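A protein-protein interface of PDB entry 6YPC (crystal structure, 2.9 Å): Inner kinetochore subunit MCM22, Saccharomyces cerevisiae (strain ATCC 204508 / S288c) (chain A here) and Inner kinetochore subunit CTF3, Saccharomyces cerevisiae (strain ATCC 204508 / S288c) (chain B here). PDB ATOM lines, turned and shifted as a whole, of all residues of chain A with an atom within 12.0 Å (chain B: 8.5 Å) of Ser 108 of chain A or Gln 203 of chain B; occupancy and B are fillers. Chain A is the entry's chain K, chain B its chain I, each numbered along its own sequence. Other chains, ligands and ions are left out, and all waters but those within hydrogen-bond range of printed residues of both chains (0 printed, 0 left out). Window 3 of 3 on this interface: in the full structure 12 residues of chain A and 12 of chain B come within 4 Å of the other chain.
The backbone carbonyl oxygen (O) of Ser 108 of chain A sits close to the side-chain amide nitrogen (NE2) of Gln 203 of chain B (2.3 Å).
OD1 of Asp 103 of chain A is in hydrogen-bond range of N of Asn 105 of chain A (2.9 Å). The backbone NH of Glu 106 of chain A lies within hydrogen-bond range of the side-chain carboxylate of Asp 103 of chain A. The side-chain carboxylate (OE2) of Glu 106 of chain A lies within hydrogen-bond range of the backbone NH (N) of Ser 108 of chain A (2.6 Å). The backbone carbonyl oxygen of Trp 166 of chain B is in hydrogen-bond range of the side-chain hydroxyl of Ser 169 of chain B (3.2 Å). O of Gln 203 of chain B sits at hydrogen-bond distance from OG of Ser 207 of chain B (2.8 Å).
Trp 166 of chain B touches Asp 103 of chain A (CB to O, 3.3 Å). O of Phe 104 of chain A touches CE of Lys 164 of chain B, at 3.3 Å. Phe 104 of chain A touches Trp 166 of chain B (CD1 to CD2, 3.6 Å). Glu 106 of chain A touches Lys 164 of chain B. Glu 106 of chain A touches Pro 165 of chain B (O to CD, 3.0 Å). Pro 165 of chain B touches Thr 107 of chain A (CD to CA, 3.9 Å). N of Ser 108 of chain A touches CG of Pro 165 of chain B (3.97 Å).
Of the printed residues of chain B, Ser 108 of chain A touches Pro 165 and Gln 203. Gln 203 of chain B touches one residue of chain A. Pro 165 of chain B touches three residues of chain A. No residue of chain A comes within 4 Å of Ile 204 of chain B. No residue of chain A comes within 4 Å of Ser 207 of chain B. Of the printed residues of chain B, Asp 103 of chain A touches Trp 166. Printed residues of chain A within 4 Å of Trp 166 of chain B: Asp 103 and Phe 104. The nearest residue of chain A that does not touch Gln 203 of chain B is Thr 107 of chain A (6.3 Å).
Of the 22 printed residues of chain B, 4 touch a printed residue of chain A. Printed residues of chain B that touch a printed residue of chain A: Lys 164, Pro 165, Trp 166 and Gln 203. Hydrophobic or aromatic side chains of chain B within 4 Å of the printed part of chain A: Pro 165 and Trp 166. Of the 7 printed residues of chain A, 5 touch a printed residue of chain B. Printed residues of chain A that touch a printed residue of chain B: Asp 103, Phe 104, Glu 106, Thr 107 and Ser 108. Among the printed residues, 8 pairs touch across the chains. Among the printed residues, no Asp or Glu carboxylate lies within 4 Å of a Lys or Arg side-chain nitrogen of the other chain.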
ATOM      1  N   ILE A 102      -9.040   6.327  15.031  1.00  0.00           N
ATOM      2  CA  ILE A 102     -10.361   6.939  15.073  1.00  0.00           C
ATOM      3  C   ILE A 102     -10.143   8.447  15.149  1.00  0.00           C
ATOM      4  O   ILE A 102      -9.026   8.905  15.429  1.00  0.00           O
ATOM      5  CB  ILE A 102     -11.188   6.425  16.260  1.00  0.00           C
ATOM      6  CG1 ILE A 102     -10.432   6.683  17.553  1.00  0.00           C
ATOM      7  CG2 ILE A 102     -11.480   4.935  16.130  1.00  0.00           C
ATOM      8  CD1 ILE A 102     -11.219   6.336  18.782  1.00  0.00           C
ATOM      9  N   ASP A 103     -11.188   9.236  14.891  1.00  0.00           N
ATOM     10  CA  ASP A 103     -11.057  10.689  14.876  1.00  0.00           C
ATOM     11  C   ASP A 103     -11.379  11.231  16.262  1.00  0.00           C
ATOM     12  O   ASP A 103     -12.509  11.094  16.745  1.00  0.00           O
ATOM     13  CB  ASP A 103     -11.965  11.305  13.819  1.00  0.00           C
ATOM     14  CG  ASP A 103     -11.572  12.735  13.472  1.00  0.00           C
ATOM     15  OD1 ASP A 103     -10.901  13.413  14.303  1.00  0.00           O
ATOM     16  OD2 ASP A 103     -11.911  13.171  12.344  1.00  0.00           O
ATOM     17  N   PHE A 104     -10.392  11.852  16.906  1.00  0.00           N
ATOM     18  CA  PHE A 104     -10.651  12.438  18.212  1.00  0.00           C
ATOM     19  C   PHE A 104     -11.064  13.893  18.133  1.00  0.00           C
ATOM     20  O   PHE A 104     -11.655  14.401  19.093  1.00  0.00           O
ATOM     21  CB  PHE A 104      -9.426  12.326  19.122  1.00  0.00           C
ATOM     22  CG  PHE A 104      -9.027  10.918  19.407  1.00  0.00           C
ATOM     23  CD1 PHE A 104      -9.771  10.142  20.271  1.00  0.00           C
ATOM     24  CD2 PHE A 104      -7.924  10.362  18.795  1.00  0.00           C
ATOM     25  CE1 PHE A 104      -9.422   8.837  20.521  1.00  0.00           C
ATOM     26  CE2 PHE A 104      -7.571   9.054  19.047  1.00  0.00           C
ATOM     27  CZ  PHE A 104      -8.321   8.292  19.913  1.00  0.00           C
ATOM     28  N   ASN A 105     -10.779  14.562  17.015  1.00  0.00           N
ATOM     29  CA  ASN A 105     -11.062  15.982  16.892  1.00  0.00           C
ATOM     30  C   ASN A 105     -12.487  16.290  16.447  1.00  0.00           C
ATOM     31  O   ASN A 105     -12.998  17.363  16.792  1.00  0.00           O
ATOM     32  CB  ASN A 105     -10.057  16.603  15.929  1.00  0.00           C
ATOM     33  CG  ASN A 105      -8.621  16.346  16.353  1.00  0.00           C
ATOM     34  OD1 ASN A 105      -8.161  16.868  17.372  1.00  0.00           O
ATOM     35  ND2 ASN A 105      -7.907  15.548  15.571  1.00  0.00           N
ATOM     36  N   GLU A 106     -13.145  15.376  15.721  1.00  0.00           N
ATOM     37  CA  GLU A 106     -14.466  15.654  15.168  1.00  0.00           C
ATOM     38  C   GLU A 106     -15.475  15.885  16.283  1.00  0.00           C
ATOM     39  O   GLU A 106     -15.357  15.331  17.377  1.00  0.00           O
ATOM     40  CB  GLU A 106     -14.936  14.516  14.252  1.00  0.00           C
ATOM     41  CG  GLU A 106     -16.315  14.760  13.563  1.00  0.00           C
ATOM     42  CD  GLU A 106     -16.502  16.196  12.994  1.00  0.00           C
ATOM     43  OE1 GLU A 106     -15.692  16.622  12.131  1.00  0.00           O
ATOM     44  OE2 GLU A 106     -17.462  16.901  13.419  1.00  0.00           O
ATOM     45  N   THR A 107     -16.465  16.746  15.994  1.00  0.00           N
ATOM     46  CA  THR A 107     -17.420  17.208  16.991  1.00  0.00           C
ATOM     47  C   THR A 107     -18.888  16.990  16.627  1.00  0.00           C
ATOM     48  O   THR A 107     -19.739  17.142  17.510  1.00  0.00           O
ATOM     49  CB  THR A 107     -17.193  18.703  17.290  1.00  0.00           C
ATOM     50  OG1 THR A 107     -17.788  19.497  16.264  1.00  0.00           O
ATOM     51  CG2 THR A 107     -15.711  19.031  17.337  1.00  0.00           C
ATOM     52  N   SER A 108     -19.217  16.638  15.383  1.00  0.00           N
ATOM     53  CA  SER A 108     -20.620  16.474  14.964  1.00  0.00           C
ATOM     54  C   SER A 108     -21.373  15.339  15.680  1.00  0.00           C
ATOM     55  O   SER A 108     -22.453  14.905  15.245  1.00  0.00           O
ATOM     56  CB  SER A 108     -20.686  16.224  13.470  1.00  0.00           C
ATOM     57  OG  SER A 108     -20.716  14.828  13.240  1.00  0.00           O
ATOM     58  N   PRO B 160     -21.667  20.200  26.515  1.00  0.00           N
ATOM     59  CA  PRO B 160     -21.649  19.460  25.240  1.00  0.00           C
ATOM     60  C   PRO B 160     -20.273  19.347  24.587  1.00  0.00           C
ATOM     61  O   PRO B 160     -20.162  18.720  23.528  1.00  0.00           O
ATOM     62  CB  PRO B 160     -22.643  20.247  24.357  1.00  0.00           C
ATOM     63  CG  PRO B 160     -22.949  21.514  25.093  1.00  0.00           C
ATOM     64  CD  PRO B 160     -22.715  21.237  26.538  1.00  0.00           C
ATOM     65  N   VAL B 163     -19.261  15.426  25.045  1.00  0.00           N
ATOM     66  CA  VAL B 163     -19.864  14.409  24.184  1.00  0.00           C
ATOM     67  C   VAL B 163     -19.390  14.625  22.739  1.00  0.00           C
ATOM     68  O   VAL B 163     -19.684  15.650  22.120  1.00  0.00           O
ATOM     69  CB  VAL B 163     -21.397  14.410  24.315  1.00  0.00           C
ATOM     70  CG1 VAL B 163     -21.946  15.806  24.196  1.00  0.00           C
ATOM     71  CG2 VAL B 163     -22.036  13.507  23.291  1.00  0.00           C
ATOM     72  N   LYS B 164     -18.628  13.668  22.215  1.00  0.00           N
ATOM     73  CA  LYS B 164     -18.009  13.707  20.895  1.00  0.00           C
ATOM     74  C   LYS B 164     -18.283  12.413  20.157  1.00  0.00           C
ATOM     75  O   LYS B 164     -18.689  11.406  20.764  1.00  0.00           O
ATOM     76  CB  LYS B 164     -16.487  13.928  20.974  1.00  0.00           C
ATOM     77  CG  LYS B 164     -16.052  15.025  21.888  1.00  0.00           C
ATOM     78  CD  LYS B 164     -14.555  15.285  21.795  1.00  0.00           C
ATOM     79  CE  LYS B 164     -14.186  16.020  20.533  1.00  0.00           C
ATOM     80  NZ  LYS B 164     -13.154  17.045  20.869  1.00  0.00           N
ATOM     81  N   PRO B 165     -18.083  12.378  18.838  1.00  0.00           N
ATOM     82  CA  PRO B 165     -18.425  11.161  18.099  1.00  0.00           C
ATOM     83  C   PRO B 165     -17.637   9.941  18.549  1.00  0.00           C
ATOM     84  O   PRO B 165     -18.214   8.854  18.704  1.00  0.00           O
ATOM     85  CB  PRO B 165     -18.123  11.542  16.645  1.00  0.00           C
ATOM     86  CG  PRO B 165     -18.220  13.003  16.619  1.00  0.00           C
ATOM     87  CD  PRO B 165     -17.694  13.466  17.926  1.00  0.00           C
ATOM     88  N   TRP B 166     -16.331  10.086  18.779  1.00  0.00           N
ATOM     89  CA  TRP B 166     -15.538   8.897  19.043  1.00  0.00           C
ATOM     90  C   TRP B 166     -15.947   8.240  20.341  1.00  0.00           C
ATOM     91  O   TRP B 166     -15.966   7.009  20.425  1.00  0.00           O
ATOM     92  CB  TRP B 166     -14.062   9.230  19.052  1.00  0.00           C
ATOM     93  CG  TRP B 166     -13.613  10.019  20.204  1.00  0.00           C
ATOM     94  CD1 TRP B 166     -13.514  11.377  20.275  1.00  0.00           C
ATOM     95  CD2 TRP B 166     -13.134   9.513  21.453  1.00  0.00           C
ATOM     96  NE1 TRP B 166     -13.015  11.748  21.503  1.00  0.00           N
ATOM     97  CE2 TRP B 166     -12.774  10.622  22.243  1.00  0.00           C
ATOM     98  CE3 TRP B 166     -12.974   8.232  21.979  1.00  0.00           C
ATOM     99  CZ2 TRP B 166     -12.272  10.491  23.536  1.00  0.00           C
ATOM    100  CZ3 TRP B 166     -12.464   8.100  23.269  1.00  0.00           C
ATOM    101  CH2 TRP B 166     -12.126   9.223  24.032  1.00  0.00           C
ATOM    102  N   LEU B 168     -18.854   7.926  21.062  1.00  0.00           N
ATOM    103  CA  LEU B 168     -20.145   7.285  20.807  1.00  0.00           C
ATOM    104  C   LEU B 168     -19.991   5.856  20.325  1.00  0.00           C
ATOM    105  O   LEU B 168     -20.714   4.953  20.776  1.00  0.00           O
ATOM    106  CB  LEU B 168     -20.948   8.089  19.791  1.00  0.00           C
ATOM    107  CG  LEU B 168     -21.367   9.413  20.419  1.00  0.00           C
ATOM    108  CD1 LEU B 168     -21.609  10.463  19.354  1.00  0.00           C
ATOM    109  CD2 LEU B 168     -22.587   9.192  21.337  1.00  0.00           C
ATOM    110  N   SER B 169     -19.075   5.638  19.395  1.00  0.00           N
ATOM    111  CA  SER B 169     -18.897   4.289  18.887  1.00  0.00           C
ATOM    112  C   SER B 169     -18.333   3.381  19.967  1.00  0.00           C
ATOM    113  O   SER B 169     -18.789   2.242  20.127  1.00  0.00           O
ATOM    114  CB  SER B 169     -17.997   4.322  17.668  1.00  0.00           C
ATOM    115  OG  SER B 169     -16.906   5.167  17.950  1.00  0.00           O
ATOM    116  N   LYS B 172     -21.179   2.462  21.443  1.00  0.00           N
ATOM    117  CA  LYS B 172     -22.111   1.645  20.676  1.00  0.00           C
ATOM    118  C   LYS B 172     -21.519   0.264  20.419  1.00  0.00           C
ATOM    119  O   LYS B 172     -22.210  -0.752  20.540  1.00  0.00           O
ATOM    120  CB  LYS B 172     -22.524   2.316  19.362  1.00  0.00           C
ATOM    121  CG  LYS B 172     -23.503   1.381  18.567  1.00  0.00           C
ATOM    122  CD  LYS B 172     -23.960   1.866  17.180  1.00  0.00           C
ATOM    123  CE  LYS B 172     -22.861   2.657  16.464  1.00  0.00           C
ATOM    124  NZ  LYS B 172     -23.069   2.872  14.978  1.00  0.00           N
ATOM    125  N   LEU B 191     -25.908   7.357  26.746  1.00  0.00           N
ATOM    126  CA  LEU B 191     -26.394   8.020  25.545  1.00  0.00           C
ATOM    127  C   LEU B 191     -27.505   9.008  25.875  1.00  0.00           C
ATOM    128  O   LEU B 191     -27.445  10.184  25.488  1.00  0.00           O
ATOM    129  CB  LEU B 191     -26.886   6.975  24.570  1.00  0.00           C
ATOM    130  CG  LEU B 191     -25.804   6.065  24.035  1.00  0.00           C
ATOM    131  CD1 LEU B 191     -26.484   5.074  23.093  1.00  0.00           C
ATOM    132  CD2 LEU B 191     -24.720   6.879  23.317  1.00  0.00           C
ATOM    133  N   GLN B 195     -27.879  12.745  24.885  1.00  0.00           N
ATOM    134  CA  GLN B 195     -29.108  13.314  24.358  1.00  0.00           C
ATOM    135  C   GLN B 195     -29.577  14.456  25.249  1.00  0.00           C
ATOM    136  O   GLN B 195     -29.679  15.610  24.806  1.00  0.00           O
ATOM    137  CB  GLN B 195     -30.170  12.213  24.242  1.00  0.00           C
ATOM    138  CG  GLN B 195     -31.551  12.704  23.896  1.00  0.00           C
ATOM    139  CD  GLN B 195     -32.002  12.175  22.567  1.00  0.00           C
ATOM    140  OE1 GLN B 195     -31.176  11.910  21.687  1.00  0.00           O
ATOM    141  NE2 GLN B 195     -33.320  12.013  22.401  1.00  0.00           N
ATOM    142  N   VAL B 198     -26.706  17.567  24.728  1.00  0.00           N
ATOM    143  CA  VAL B 198     -26.356  18.276  23.502  1.00  0.00           C
ATOM    144  C   VAL B 198     -27.580  18.569  22.633  1.00  0.00           C
ATOM    145  O   VAL B 198     -27.516  19.440  21.746  1.00  0.00           O
ATOM    146  CB  VAL B 198     -25.309  17.462  22.723  1.00  0.00           C
ATOM    147  CG1 VAL B 198     -25.957  16.236  22.085  1.00  0.00           C
ATOM    148  CG2 VAL B 198     -24.611  18.323  21.698  1.00  0.00           C
ATOM    149  N   ALA B 200     -30.332  17.556  19.816  1.00  0.00           N
ATOM    150  CA  ALA B 200     -30.761  16.692  18.717  1.00  0.00           C
ATOM    151  C   ALA B 200     -29.764  15.579  18.405  1.00  0.00           C
ATOM    152  O   ALA B 200     -29.963  14.426  18.814  1.00  0.00           O
ATOM    153  CB  ALA B 200     -31.000  17.526  17.455  1.00  0.00           C
ATOM    154  N   SER B 201     -28.693  15.938  17.684  1.00  0.00           N
ATOM    155  CA  SER B 201     -27.673  15.054  17.121  1.00  0.00           C
ATOM    156  C   SER B 201     -28.237  13.724  16.616  1.00  0.00           C
ATOM    157  O   SER B 201     -28.582  12.822  17.396  1.00  0.00           O
ATOM    158  CB  SER B 201     -26.553  14.787  18.127  1.00  0.00           C
ATOM    159  OG  SER B 201     -25.760  13.679  17.701  1.00  0.00           O
ATOM    160  N   SER B 202     -28.284  13.592  15.287  1.00  0.00           N
ATOM    161  CA  SER B 202     -28.853  12.401  14.661  1.00  0.00           C
ATOM    162  C   SER B 202     -28.144  11.126  15.102  1.00  0.00           C
ATOM    163  O   SER B 202     -28.796  10.108  15.377  1.00  0.00           O
ATOM    164  CB  SER B 202     -28.794  12.540  13.138  1.00  0.00           C
ATOM    165  OG  SER B 202     -29.163  11.327  12.509  1.00  0.00           O
ATOM    166  N   GLN B 203     -26.807  11.166  15.164  1.00  0.00           N
ATOM    167  CA  GLN B 203     -26.033   9.965  15.461  1.00  0.00           C
ATOM    168  C   GLN B 203     -26.492   9.308  16.753  1.00  0.00           C
ATOM    169  O   GLN B 203     -26.789   8.109  16.784  1.00  0.00           O
ATOM    170  CB  GLN B 203     -24.560  10.313  15.550  1.00  0.00           C
ATOM    171  CG  GLN B 203     -23.924  10.543  14.213  1.00  0.00           C
ATOM    172  CD  GLN B 203     -22.916  11.660  14.264  1.00  0.00           C
ATOM    173  OE1 GLN B 203     -21.758  11.466  13.899  1.00  0.00           O
ATOM    174  NE2 GLN B 203     -23.352  12.851  14.728  1.00  0.00           N
ATOM    175  N   ILE B 204     -26.569  10.084  17.830  1.00  0.00           N
ATOM    176  CA  ILE B 204     -26.944   9.523  19.123  1.00  0.00           C
ATOM    177  C   ILE B 204     -28.319   8.875  19.045  1.00  0.00           C
ATOM    178  O   ILE B 204     -28.509   7.711  19.427  1.00  0.00           O
ATOM    179  CB  ILE B 204     -26.915  10.609  20.208  1.00  0.00           C
ATOM    180  CG1 ILE B 204     -25.521  11.233  20.299  1.00  0.00           C
ATOM    181  CG2 ILE B 204     -27.432  10.025  21.548  1.00  0.00           C
ATOM    182  CD1 ILE B 204     -25.414  12.356  21.322  1.00  0.00           C
ATOM    183  N   THR B 205     -29.302   9.620  18.552  1.00  0.00           N
ATOM    184  CA  THR B 205     -30.668   9.147  18.693  1.00  0.00           C
ATOM    185  C   THR B 205     -30.865   7.836  17.945  1.00  0.00           C
ATOM    186  O   THR B 205     -31.496   6.910  18.463  1.00  0.00           O
ATOM    187  CB  THR B 205     -31.655  10.226  18.245  1.00  0.00           C
ATOM    188  OG1 THR B 205     -32.978   9.679  18.241  1.00  0.00           O
ATOM    189  CG2 THR B 205     -31.294  10.771  16.870  1.00  0.00           C
ATOM    190  N   GLU B 206     -30.249   7.694  16.771  1.00  0.00           N
ATOM    191  CA  GLU B 206     -30.403   6.430  16.057  1.00  0.00           C
ATOM    192  C   GLU B 206     -29.577   5.305  16.680  1.00  0.00           C
ATOM    193  O   GLU B 206     -29.959   4.133  16.575  1.00  0.00           O
ATOM    194  CB  GLU B 206     -30.062   6.604  14.585  1.00  0.00           C
ATOM    195  CG  GLU B 206     -28.736   7.259  14.316  1.00  0.00           C
ATOM    196  CD  GLU B 206     -28.234   6.953  12.913  1.00  0.00           C
ATOM    197  OE1 GLU B 206     -27.001   6.978  12.686  1.00  0.00           O
ATOM    198  OE2 GLU B 206     -29.087   6.674  12.037  1.00  0.00           O
ATOM    199  N   SER B 207     -28.457   5.621  17.331  1.00  0.00           N
ATOM    200  CA  SER B 207     -27.762   4.582  18.084  1.00  0.00           C
ATOM    201  C   SER B 207     -28.683   3.974  19.119  1.00  0.00           C
ATOM    202  O   SER B 207     -28.754   2.746  19.256  1.00  0.00           O
ATOM    203  CB  SER B 207     -26.523   5.135  18.774  1.00  0.00           C
ATOM    204  OG  SER B 207     -25.685   5.789  17.853  1.00  0.00           O
ATOM    205  N   ILE B 208     -29.412   4.823  19.848  1.00  0.00           N
ATOM    206  CA  ILE B 208     -30.274   4.308  20.903  1.00  0.00           C
ATOM    207  C   ILE B 208     -31.279   3.332  20.321  1.00  0.00           C
ATOM    208  O   ILE B 208     -31.612   2.320  20.946  1.00  0.00           O
ATOM    209  CB  ILE B 208     -30.959   5.459  21.670  1.00  0.00           C
ATOM    210  CG1 ILE B 208     -29.926   6.512  22.062  1.00  0.00           C
ATOM    211  CG2 ILE B 208     -31.574   4.927  22.927  1.00  0.00           C
ATOM    212  CD1 ILE B 208     -30.386   7.495  23.069  1.00  0.00           C
ATOM    213  N   ILE B 209     -31.736   3.587  19.099  1.00  0.00           N
ATOM    214  CA  ILE B 209     -32.689   2.685  18.469  1.00  0.00           C
ATOM    215  C   ILE B 209     -32.044   1.333  18.190  1.00  0.00           C
ATOM    216  O   ILE B 209     -32.594   0.284  18.545  1.00  0.00           O
ATOM    217  CB  ILE B 209     -33.245   3.329  17.192  1.00  0.00           C
ATOM    218  CG1 ILE B 209     -34.049   4.566  17.559  1.00  0.00           C
ATOM    219  CG2 ILE B 209     -34.102   2.349  16.439  1.00  0.00           C
ATOM    220  CD1 ILE B 209     -33.685   5.759  16.777  1.00  0.00           C
ATOM    221  N   THR B 210     -30.860   1.344  17.558  1.00  0.00           N
ATOM    222  CA  THR B 210     -30.106   0.129  17.246  1.00  0.00           C
ATOM    223  C   THR B 210     -29.885  -0.772  18.458  1.00  0.00           C
ATOM    224  O   THR B 210     -29.691  -1.981  18.299  1.00  0.00           O
ATOM    225  CB  THR B 210     -28.751   0.513  16.644  1.00  0.00           C
ATOM    226  OG1 THR B 210     -28.913   1.664  15.803  1.00  0.00           O
ATOM    227  CG2 THR B 210     -28.177  -0.634  15.835  1.00  0.00           C
